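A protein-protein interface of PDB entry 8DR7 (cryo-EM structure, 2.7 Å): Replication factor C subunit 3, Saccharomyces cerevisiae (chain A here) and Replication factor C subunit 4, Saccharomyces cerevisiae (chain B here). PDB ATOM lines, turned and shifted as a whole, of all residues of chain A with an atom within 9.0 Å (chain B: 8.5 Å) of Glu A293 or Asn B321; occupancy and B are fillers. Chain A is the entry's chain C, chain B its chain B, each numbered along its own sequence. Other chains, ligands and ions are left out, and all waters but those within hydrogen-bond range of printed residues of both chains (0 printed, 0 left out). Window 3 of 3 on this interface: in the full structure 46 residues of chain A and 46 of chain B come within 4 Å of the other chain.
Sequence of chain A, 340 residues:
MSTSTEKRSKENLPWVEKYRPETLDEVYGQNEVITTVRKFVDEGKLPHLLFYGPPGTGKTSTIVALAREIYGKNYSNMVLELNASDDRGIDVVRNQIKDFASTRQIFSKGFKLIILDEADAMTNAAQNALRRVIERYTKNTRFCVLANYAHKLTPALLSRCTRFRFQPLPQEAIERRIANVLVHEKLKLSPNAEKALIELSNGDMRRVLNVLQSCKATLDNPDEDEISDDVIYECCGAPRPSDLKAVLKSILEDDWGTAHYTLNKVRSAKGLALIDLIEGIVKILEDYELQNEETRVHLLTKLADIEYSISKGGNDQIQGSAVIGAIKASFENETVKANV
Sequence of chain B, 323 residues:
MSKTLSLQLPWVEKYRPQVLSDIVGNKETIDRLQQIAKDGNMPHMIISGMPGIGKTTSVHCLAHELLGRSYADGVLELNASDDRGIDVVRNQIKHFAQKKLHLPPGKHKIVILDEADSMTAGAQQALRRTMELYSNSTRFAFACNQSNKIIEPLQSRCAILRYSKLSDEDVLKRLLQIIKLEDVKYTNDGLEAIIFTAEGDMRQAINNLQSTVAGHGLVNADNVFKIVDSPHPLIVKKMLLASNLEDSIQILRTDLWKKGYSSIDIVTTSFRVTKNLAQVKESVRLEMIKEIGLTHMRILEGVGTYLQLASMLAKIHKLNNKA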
ATOM      1  N   LEU A 290      17.139   4.730 -33.236  1.00  0.00           N
ATOM      2  CA  LEU A 290      16.540   3.799 -32.291  1.00  0.00           C
ATOM      3  C   LEU A 290      15.052   4.088 -32.119  1.00  0.00           C
ATOM      4  O   LEU A 290      14.603   5.234 -32.198  1.00  0.00           O
ATOM      5  CB  LEU A 290      17.246   3.883 -30.938  1.00  0.00           C
ATOM      6  CG  LEU A 290      18.722   3.484 -30.932  1.00  0.00           C
ATOM      7  CD1 LEU A 290      19.373   3.876 -29.615  1.00  0.00           C
ATOM      8  CD2 LEU A 290      18.880   1.994 -31.188  1.00  0.00           C
ATOM      9  N   GLN A 291      14.284   3.023 -31.880  1.00  0.00           N
ATOM     10  CA  GLN A 291      12.847   3.137 -31.672  1.00  0.00           C
ATOM     11  C   GLN A 291      12.458   3.297 -30.209  1.00  0.00           C
ATOM     12  O   GLN A 291      11.291   3.592 -29.927  1.00  0.00           O
ATOM     13  CB  GLN A 291      12.132   1.905 -32.239  1.00  0.00           C
ATOM     14  CG  GLN A 291      12.160   1.815 -33.757  1.00  0.00           C
ATOM     15  CD  GLN A 291      10.889   1.222 -34.339  1.00  0.00           C
ATOM     16  OE1 GLN A 291       9.942   0.913 -33.614  1.00  0.00           O
ATOM     17  NE2 GLN A 291      10.863   1.061 -35.656  1.00  0.00           N
ATOM     18  N   ASN A 292      13.393   3.112 -29.280  1.00  0.00           N
ATOM     19  CA  ASN A 292      13.111   3.184 -27.854  1.00  0.00           C
ATOM     20  C   ASN A 292      14.158   4.047 -27.165  1.00  0.00           C
ATOM     21  O   ASN A 292      15.269   4.215 -27.677  1.00  0.00           O
ATOM     22  CB  ASN A 292      13.083   1.785 -27.227  1.00  0.00           C
ATOM     23  CG  ASN A 292      11.963   0.924 -27.771  1.00  0.00           C
ATOM     24  OD1 ASN A 292      10.939   1.430 -28.230  1.00  0.00           O
ATOM     25  ND2 ASN A 292      12.150  -0.390 -27.718  1.00  0.00           N
ATOM     26  N   GLU A 293      13.794   4.592 -26.003  1.00  0.00           N
ATOM     27  CA  GLU A 293      14.696   5.480 -25.274  1.00  0.00           C
ATOM     28  C   GLU A 293      15.546   4.722 -24.259  1.00  0.00           C
ATOM     29  O   GLU A 293      16.758   4.955 -24.165  1.00  0.00           O
ATOM     30  CB  GLU A 293      13.891   6.575 -24.575  1.00  0.00           C
ATOM     31  CG  GLU A 293      14.739   7.616 -23.870  1.00  0.00           C
ATOM     32  CD  GLU A 293      13.918   8.769 -23.334  1.00  0.00           C
ATOM     33  OE1 GLU A 293      13.104   9.326 -24.100  1.00  0.00           O
ATOM     34  OE2 GLU A 293      14.082   9.115 -22.144  1.00  0.00           O
ATOM     35  N   GLU A 294      14.931   3.825 -23.482  1.00  0.00           N
ATOM     36  CA  GLU A 294      15.679   3.085 -22.472  1.00  0.00           C
ATOM     37  C   GLU A 294      16.845   2.309 -23.071  1.00  0.00           C
ATOM     38  O   GLU A 294      17.838   2.087 -22.374  1.00  0.00           O
ATOM     39  CB  GLU A 294      14.781   2.108 -21.699  1.00  0.00           C
ATOM     40  CG  GLU A 294      14.088   0.973 -22.488  1.00  0.00           C
ATOM     41  CD  GLU A 294      13.226   1.408 -23.659  1.00  0.00           C
ATOM     42  OE1 GLU A 294      12.496   0.544 -24.191  1.00  0.00           O
ATOM     43  OE2 GLU A 294      13.254   2.595 -24.041  1.00  0.00           O
ATOM     44  N   THR A 295      16.757   1.890 -24.336  1.00  0.00           N
ATOM     45  CA  THR A 295      17.898   1.233 -24.967  1.00  0.00           C
ATOM     46  C   THR A 295      19.090   2.181 -25.049  1.00  0.00           C
ATOM     47  O   THR A 295      20.219   1.812 -24.701  1.00  0.00           O
ATOM     48  CB  THR A 295      17.526   0.719 -26.364  1.00  0.00           C
ATOM     49  OG1 THR A 295      18.716   0.356 -27.074  1.00  0.00           O
ATOM     50  CG2 THR A 295      16.776   1.773 -27.174  1.00  0.00           C
ATOM     51  N   ARG A 296      18.851   3.418 -25.491  1.00  0.00           N
ATOM     52  CA  ARG A 296      19.924   4.404 -25.540  1.00  0.00           C
ATOM     53  C   ARG A 296      20.423   4.733 -24.142  1.00  0.00           C
ATOM     54  O   ARG A 296      21.628   4.918 -23.930  1.00  0.00           O
ATOM     55  CB  ARG A 296      19.441   5.673 -26.245  1.00  0.00           C
ATOM     56  CG  ARG A 296      20.519   6.734 -26.410  1.00  0.00           C
ATOM     57  CD  ARG A 296      20.147   7.758 -27.469  1.00  0.00           C
ATOM     58  NE  ARG A 296      20.178   7.199 -28.816  1.00  0.00           N
ATOM     59  CZ  ARG A 296      21.281   7.022 -29.530  1.00  0.00           C
ATOM     60  NH1 ARG A 296      22.474   7.343 -29.055  1.00  0.00           N
ATOM     61  NH2 ARG A 296      21.186   6.510 -30.754  1.00  0.00           N
ATOM     62  N   VAL A 297      19.510   4.820 -23.173  1.00  0.00           N
ATOM     63  CA  VAL A 297      19.913   5.115 -21.801  1.00  0.00           C
ATOM     64  C   VAL A 297      20.856   4.035 -21.286  1.00  0.00           C
ATOM     65  O   VAL A 297      21.914   4.326 -20.713  1.00  0.00           O
ATOM     66  CB  VAL A 297      18.674   5.258 -20.899  1.00  0.00           C
ATOM     67  CG1 VAL A 297      19.092   5.439 -19.448  1.00  0.00           C
ATOM     68  CG2 VAL A 297      17.809   6.421 -21.360  1.00  0.00           C
ATOM     69  N   HIS A 298      20.483   2.767 -21.482  1.00  0.00           N
ATOM     70  CA  HIS A 298      21.328   1.667 -21.036  1.00  0.00           C
ATOM     71  C   HIS A 298      22.666   1.674 -21.760  1.00  0.00           C
ATOM     72  O   HIS A 298      23.718   1.498 -21.133  1.00  0.00           O
ATOM     73  CB  HIS A 298      20.610   0.335 -21.253  1.00  0.00           C
ATOM     74  CG  HIS A 298      19.433   0.131 -20.351  1.00  0.00           C
ATOM     75  ND1 HIS A 298      18.174  -0.166 -20.828  1.00  0.00           N
ATOM     76  CD2 HIS A 298      19.323   0.178 -19.003  1.00  0.00           C
ATOM     77  CE1 HIS A 298      17.339  -0.292 -19.811  1.00  0.00           C
ATOM     78  NE2 HIS A 298      18.012  -0.087 -18.693  1.00  0.00           N
ATOM     79  N   LEU A 299      22.649   1.874 -23.080  1.00  0.00           N
ATOM     80  CA  LEU A 299      23.901   1.938 -23.827  1.00  0.00           C
ATOM     81  C   LEU A 299      24.824   2.998 -23.244  1.00  0.00           C
ATOM     82  O   LEU A 299      25.986   2.721 -22.921  1.00  0.00           O
ATOM     83  CB  LEU A 299      23.621   2.232 -25.302  1.00  0.00           C
ATOM     84  CG  LEU A 299      23.644   1.041 -26.261  1.00  0.00           C
ATOM     85  CD1 LEU A 299      23.032   1.423 -27.599  1.00  0.00           C
ATOM     86  CD2 LEU A 299      25.064   0.526 -26.449  1.00  0.00           C
ATOM     87  N   LEU A 300      24.314   4.221 -23.084  1.00  0.00           N
ATOM     88  CA  LEU A 300      25.149   5.317 -22.610  1.00  0.00           C
ATOM     89  C   LEU A 300      25.674   5.039 -21.208  1.00  0.00           C
ATOM     90  O   LEU A 300      26.870   5.199 -20.938  1.00  0.00           O
ATOM     91  CB  LEU A 300      24.357   6.626 -22.638  1.00  0.00           C
ATOM     92  CG  LEU A 300      24.485   7.484 -23.901  1.00  0.00           C
ATOM     93  CD1 LEU A 300      25.911   7.985 -24.079  1.00  0.00           C
ATOM     94  CD2 LEU A 300      24.031   6.716 -25.134  1.00  0.00           C
ATOM     95  N   THR A 301      24.795   4.608 -20.298  1.00  0.00           N
ATOM     96  CA  THR A 301      25.213   4.396 -18.917  1.00  0.00           C
ATOM     97  C   THR A 301      26.263   3.295 -18.822  1.00  0.00           C
ATOM     98  O   THR A 301      27.301   3.463 -18.169  1.00  0.00           O
ATOM     99  CB  THR A 301      24.001   4.057 -18.048  1.00  0.00           C
ATOM    100  OG1 THR A 301      23.281   2.961 -18.628  1.00  0.00           O
ATOM    101  CG2 THR A 301      23.079   5.261 -17.922  1.00  0.00           C
ATOM    102  N   SER A 330      21.333  -3.948 -24.305  1.00  0.00           N
ATOM    103  CA  SER A 330      20.665  -2.702 -24.659  1.00  0.00           C
ATOM    104  C   SER A 330      19.856  -2.857 -25.938  1.00  0.00           C
ATOM    105  O   SER A 330      18.726  -2.363 -26.030  1.00  0.00           O
ATOM    106  CB  SER A 330      21.696  -1.584 -24.808  1.00  0.00           C
ATOM    107  OG  SER A 330      22.466  -1.440 -23.628  1.00  0.00           O
ATOM    108  N   ASN A 333      16.239  -4.616 -25.984  1.00  0.00           N
ATOM    109  CA  ASN A 333      15.018  -3.871 -25.705  1.00  0.00           C
ATOM    110  C   ASN A 333      14.313  -3.408 -26.973  1.00  0.00           C
ATOM    111  O   ASN A 333      13.131  -3.053 -26.915  1.00  0.00           O
ATOM    112  CB  ASN A 333      15.331  -2.662 -24.820  1.00  0.00           C
ATOM    113  CG  ASN A 333      15.623  -3.051 -23.383  1.00  0.00           C
ATOM    114  OD1 ASN A 333      15.022  -3.981 -22.846  1.00  0.00           O
ATOM    115  ND2 ASN A 333      16.548  -2.338 -22.754  1.00  0.00           N
ATOM    116  N   GLU A 334      15.008  -3.399 -28.114  1.00  0.00           N
ATOM    117  CA  GLU A 334      14.375  -2.965 -29.356  1.00  0.00           C
ATOM    118  C   GLU A 334      13.214  -3.878 -29.732  1.00  0.00           C
ATOM    119  O   GLU A 334      12.150  -3.402 -30.145  1.00  0.00           O
ATOM    120  CB  GLU A 334      15.408  -2.924 -30.481  1.00  0.00           C
ATOM    121  CG  GLU A 334      16.458  -1.838 -30.315  1.00  0.00           C
ATOM    122  CD  GLU A 334      15.893  -0.449 -30.528  1.00  0.00           C
ATOM    123  OE1 GLU A 334      15.304   0.107 -29.577  1.00  0.00           O
ATOM    124  OE2 GLU A 334      16.037   0.089 -31.646  1.00  0.00           O
ATOM    125  N   ALA B 242      14.426  19.417 -21.032  1.00  0.00           N
ATOM    126  CA  ALA B 242      13.935  18.831 -22.271  1.00  0.00           C
ATOM    127  C   ALA B 242      12.989  17.674 -21.978  1.00  0.00           C
ATOM    128  O   ALA B 242      13.246  16.846 -21.101  1.00  0.00           O
ATOM    129  CB  ALA B 242      15.103  18.350 -23.130  1.00  0.00           C
ATOM    130  N   SER B 243      11.883  17.624 -22.724  1.00  0.00           N
ATOM    131  CA  SER B 243      10.901  16.565 -22.518  1.00  0.00           C
ATOM    132  C   SER B 243      11.480  15.195 -22.852  1.00  0.00           C
ATOM    133  O   SER B 243      11.236  14.220 -22.132  1.00  0.00           O
ATOM    134  CB  SER B 243       9.655  16.838 -23.358  1.00  0.00           C
ATOM    135  OG  SER B 243      10.002  17.188 -24.687  1.00  0.00           O
ATOM    136  N   ASN B 244      12.246  15.102 -23.936  1.00  0.00           N
ATOM    137  CA  ASN B 244      12.805  13.842 -24.401  1.00  0.00           C
ATOM    138  C   ASN B 244      14.325  13.879 -24.313  1.00  0.00           C
ATOM    139  O   ASN B 244      14.949  14.942 -24.351  1.00  0.00           O
ATOM    140  CB  ASN B 244      12.375  13.544 -25.843  1.00  0.00           C
ATOM    141  CG  ASN B 244      10.998  14.089 -26.165  1.00  0.00           C
ATOM    142  OD1 ASN B 244      10.844  15.263 -26.503  1.00  0.00           O
ATOM    143  ND2 ASN B 244       9.985  13.235 -26.064  1.00  0.00           N
ATOM    144  N   LEU B 245      14.917  12.687 -24.194  1.00  0.00           N
ATOM    145  CA  LEU B 245      16.370  12.585 -24.122  1.00  0.00           C
ATOM    146  C   LEU B 245      17.031  13.051 -25.412  1.00  0.00           C
ATOM    147  O   LEU B 245      18.120  13.636 -25.372  1.00  0.00           O
ATOM    148  CB  LEU B 245      16.776  11.143 -23.811  1.00  0.00           C
ATOM    149  CG  LEU B 245      18.278  10.866 -23.696  1.00  0.00           C
ATOM    150  CD1 LEU B 245      18.910  11.730 -22.616  1.00  0.00           C
ATOM    151  CD2 LEU B 245      18.525   9.392 -23.419  1.00  0.00           C
ATOM    152  N   GLU B 246      16.397  12.798 -26.560  1.00  0.00           N
ATOM    153  CA  GLU B 246      16.987  13.197 -27.832  1.00  0.00           C
ATOM    154  C   GLU B 246      17.171  14.707 -27.902  1.00  0.00           C
ATOM    155  O   GLU B 246      18.207  15.192 -28.371  1.00  0.00           O
ATOM    156  CB  GLU B 246      16.110  12.714 -28.990  1.00  0.00           C
ATOM    157  CG  GLU B 246      16.305  11.254 -29.423  1.00  0.00           C
ATOM    158  CD  GLU B 246      17.724  10.746 -29.248  1.00  0.00           C
ATOM    159  OE1 GLU B 246      17.947   9.901 -28.354  1.00  0.00           O
ATOM    160  OE2 GLU B 246      18.615  11.191 -30.001  1.00  0.00           O
ATOM    161  N   ASP B 247      16.173  15.468 -27.449  1.00  0.00           N
ATOM    162  CA  ASP B 247      16.286  16.923 -27.478  1.00  0.00           C
ATOM    163  C   ASP B 247      17.428  17.405 -26.593  1.00  0.00           C
ATOM    164  O   ASP B 247      18.196  18.292 -26.984  1.00  0.00           O
ATOM    165  CB  ASP B 247      14.966  17.557 -27.042  1.00  0.00           C
ATOM    166  CG  ASP B 247      13.805  17.157 -27.930  1.00  0.00           C
ATOM    167  OD1 ASP B 247      13.469  15.954 -27.966  1.00  0.00           O
ATOM    168  OD2 ASP B 247      13.228  18.044 -28.594  1.00  0.00           O
ATOM    169  N   SER B 248      17.557  16.833 -25.393  1.00  0.00           N
ATOM    170  CA  SER B 248      18.642  17.229 -24.501  1.00  0.00           C
ATOM    171  C   SER B 248      20.000  16.899 -25.107  1.00  0.00           C
ATOM    172  O   SER B 248      20.934  17.708 -25.036  1.00  0.00           O
ATOM    173  CB  SER B 248      18.483  16.542 -23.145  1.00  0.00           C
ATOM    174  OG  SER B 248      18.274  15.149 -23.299  1.00  0.00           O
ATOM    175  N   VAL B 284      13.379  15.388  -6.415  1.00  0.00           N
ATOM    176  CA  VAL B 284      13.918  15.155  -7.751  1.00  0.00           C
ATOM    177  C   VAL B 284      15.165  16.000  -7.965  1.00  0.00           C
ATOM    178  O   VAL B 284      16.151  15.546  -8.561  1.00  0.00           O
ATOM    179  CB  VAL B 284      12.847  15.445  -8.820  1.00  0.00           C
ATOM    180  CG1 VAL B 284      13.385  15.132 -10.206  1.00  0.00           C
ATOM    181  CG2 VAL B 284      11.583  14.643  -8.540  1.00  0.00           C
ATOM    182  N   LEU B 313      22.981  12.900 -18.608  1.00  0.00           N
ATOM    183  CA  LEU B 313      21.682  13.351 -19.098  1.00  0.00           C
ATOM    184  C   LEU B 313      20.692  12.195 -19.163  1.00  0.00           C
ATOM    185  O   LEU B 313      19.519  12.348 -18.798  1.00  0.00           O
ATOM    186  CB  LEU B 313      21.837  14.002 -20.472  1.00  0.00           C
ATOM    187  CG  LEU B 313      22.443  15.407 -20.507  1.00  0.00           C
ATOM    188  CD1 LEU B 313      22.515  15.910 -21.939  1.00  0.00           C
ATOM    189  CD2 LEU B 313      21.650  16.376 -19.643  1.00  0.00           C
ATOM    190  N   ALA B 314      21.143  11.029 -19.630  1.00  0.00           N
ATOM    191  CA  ALA B 314      20.261   9.869 -19.699  1.00  0.00           C
ATOM    192  C   ALA B 314      19.796   9.449 -18.310  1.00  0.00           C
ATOM    193  O   ALA B 314      18.619   9.124 -18.112  1.00  0.00           O
ATOM    194  CB  ALA B 314      20.972   8.712 -20.400  1.00  0.00           C
ATOM    195  N   LYS B 315      20.707   9.445 -17.336  1.00  0.00           N
ATOM    196  CA  LYS B 315      20.329   9.085 -15.972  1.00  0.00           C
ATOM    197  C   LYS B 315      19.351  10.095 -15.387  1.00  0.00           C
ATOM    198  O   LYS B 315      18.404   9.717 -14.688  1.00  0.00           O
ATOM    199  CB  LYS B 315      21.576   8.972 -15.096  1.00  0.00           C
ATOM    200  CG  LYS B 315      22.399   7.722 -15.360  1.00  0.00           C
ATOM    201  CD  LYS B 315      23.471   7.523 -14.303  1.00  0.00           C
ATOM    202  CE  LYS B 315      24.316   6.295 -14.599  1.00  0.00           C
ATOM    203  NZ  LYS B 315      25.380   6.085 -13.580  1.00  0.00           N
ATOM    204  N   ILE B 316      19.564  11.384 -15.658  1.00  0.00           N
ATOM    205  CA  ILE B 316      18.637  12.404 -15.174  1.00  0.00           C
ATOM    206  C   ILE B 316      17.259  12.195 -15.785  1.00  0.00           C
ATOM    207  O   ILE B 316      16.235  12.294 -15.096  1.00  0.00           O
ATOM    208  CB  ILE B 316      19.186  13.810 -15.476  1.00  0.00           C
ATOM    209  CG1 ILE B 316      20.317  14.155 -14.504  1.00  0.00           C
ATOM    210  CG2 ILE B 316      18.074  14.848 -15.387  1.00  0.00           C
ATOM    211  CD1 ILE B 316      21.177  15.318 -14.952  1.00  0.00           C
ATOM    212  N   HIS B 317      17.207  11.906 -17.087  1.00  0.00           N
ATOM    213  CA  HIS B 317      15.924  11.658 -17.735  1.00  0.00           C
ATOM    214  C   HIS B 317      15.240  10.431 -17.144  1.00  0.00           C
ATOM    215  O   HIS B 317      14.022  10.434 -16.928  1.00  0.00           O
ATOM    216  CB  HIS B 317      16.120  11.489 -19.241  1.00  0.00           C
ATOM    217  CG  HIS B 317      15.879  12.743 -20.023  1.00  0.00           C
ATOM    218  ND1 HIS B 317      16.755  13.806 -20.014  1.00  0.00           N
ATOM    219  CD2 HIS B 317      14.859  13.104 -20.837  1.00  0.00           C
ATOM    220  CE1 HIS B 317      16.287  14.767 -20.788  1.00  0.00           C
ATOM    221  NE2 HIS B 317      15.137  14.367 -21.300  1.00  0.00           N
ATOM    222  N   LYS B 318      16.007   9.372 -16.875  1.00  0.00           N
ATOM    223  CA  LYS B 318      15.429   8.186 -16.250  1.00  0.00           C
ATOM    224  C   LYS B 318      14.868   8.515 -14.873  1.00  0.00           C
ATOM    225  O   LYS B 318      13.785   8.043 -14.505  1.00  0.00           O
ATOM    226  CB  LYS B 318      16.482   7.080 -16.149  1.00  0.00           C
ATOM    227  CG  LYS B 318      15.991   5.806 -15.468  1.00  0.00           C
ATOM    228  CD  LYS B 318      17.135   4.844 -15.182  1.00  0.00           C
ATOM    229  CE  LYS B 318      17.558   4.089 -16.430  1.00  0.00           C
ATOM    230  NZ  LYS B 318      18.611   3.077 -16.140  1.00  0.00           N
ATOM    231  N   LEU B 319      15.592   9.323 -14.095  1.00  0.00           N
ATOM    232  CA  LEU B 319      15.112   9.695 -12.768  1.00  0.00           C
ATOM    233  C   LEU B 319      13.805  10.471 -12.855  1.00  0.00           C
ATOM    234  O   LEU B 319      12.884  10.242 -12.061  1.00  0.00           O
ATOM    235  CB  LEU B 319      16.175  10.520 -12.041  1.00  0.00           C
ATOM    236  CG  LEU B 319      17.184   9.753 -11.184  1.00  0.00           C
ATOM    237  CD1 LEU B 319      18.196  10.717 -10.586  1.00  0.00           C
ATOM    238  CD2 LEU B 319      16.489   8.958 -10.086  1.00  0.00           C
ATOM    239  N   ASN B 320      13.703  11.389 -13.811  1.00  0.00           N
ATOM    240  CA  ASN B 320      12.495  12.192 -14.001  1.00  0.00           C
ATOM    241  C   ASN B 320      11.527  11.516 -14.967  1.00  0.00           C
ATOM    242  O   ASN B 320      11.097  12.096 -15.964  1.00  0.00           O
ATOM    243  CB  ASN B 320      12.876  13.585 -14.489  1.00  0.00           C
ATOM    244  CG  ASN B 320      11.926  14.657 -13.992  1.00  0.00           C
ATOM    245  OD1 ASN B 320      10.828  14.362 -13.522  1.00  0.00           O
ATOM    246  ND2 ASN B 320      12.347  15.913 -14.094  1.00  0.00           N
ATOM    247  N   ASN B 321      11.175  10.269 -14.669  1.00  0.00           N
ATOM    248  CA  ASN B 321      10.257   9.508 -15.507  1.00  0.00           C
ATOM    249  C   ASN B 321       9.485   8.490 -14.674  1.00  0.00           C
ATOM    250  O   ASN B 321      10.042   7.487 -14.229  1.00  0.00           O
ATOM    251  CB  ASN B 321      11.018   8.799 -16.629  1.00  0.00           C
ATOM    252  CG  ASN B 321      11.062   9.609 -17.911  1.00  0.00           C
ATOM    253  OD1 ASN B 321      10.148  10.381 -18.205  1.00  0.00           O
ATOM    254  ND2 ASN B 321      12.130   9.439 -18.682  1.00  0.00           N
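The side-chain carboxylate (OE1) of Glu B246 is in salt-bridge range of the guanidinium group (NE) of Arg A296, at 3.5 Å.
The backbone carbonyl oxygen (O) of Leu B245 is in hydrogen-bond range of the side-chain hydroxyl (OG) of Ser B248 (2.6 Å).
A ring nitrogen (NE2) of His B317 lies within hydrogen-bond range of the backbone NH (N) of Leu B245, 3.4 Å away.
O of His B317 is in hydrogen-bond range of ND2 of Asn B321 (2.8 Å).
The side-chain hydroxyl (OG1) of Thr A301 sits at hydrogen-bond distance from the backbone carbonyl oxygen (O) of Val A297 (2.8 Å).
The backbone carbonyl oxygen (O) of His A298 sits at hydrogen-bond distance from the side-chain hydroxyl (OG1) of Thr A301, at 2.9 Å.
Among the printed residues, merely in contact across the chains: Glu A293 with Leu B245, Glu A293 with Asn B321, Val A297 with Leu B245, Val A297 with Ala B314, Val A297 with Lys B318 and Thr A301 with Lys B315.
Printed residues of chain B within 4 Å of Glu A293: Leu B245 (3.7 Å) and Asn B321 (3.99 Å).
Of the printed residues of chain A, Asn B321 touches Glu A293.
Of the printed residues of chain B, Arg A296 touches Glu B246 (3.2 Å).
Printed residues of chain B within 4 Å of Thr A301: Lys B315.
Of the printed residues of chain A, Leu B245 touches Glu A293 (3.7 Å) and Val A297 (3.7 Å).
Of the printed residues of chain A, Lys B318 touches Val A297 (3.6 Å).
Of the printed residues of chain A, Lys B315 touches Thr A301.
Asn A292 touches none of the printed residues of chain B.
The nearest printed residue of chain A that does not touch Ala B314 is Leu A300 (4.6 Å).
Along chain B the printed residues that touch a printed residue of chain A span positions 245 to 321.
Hydrophobic or aromatic side chains of chain A that line the printed part of chain B: Val A297.
Among the printed residues, Asp or Glu carboxylates within 4 Å of a Lys or Arg side-chain nitrogen of the other chain: Arg A296 with Glu B246 (3.5 Å).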
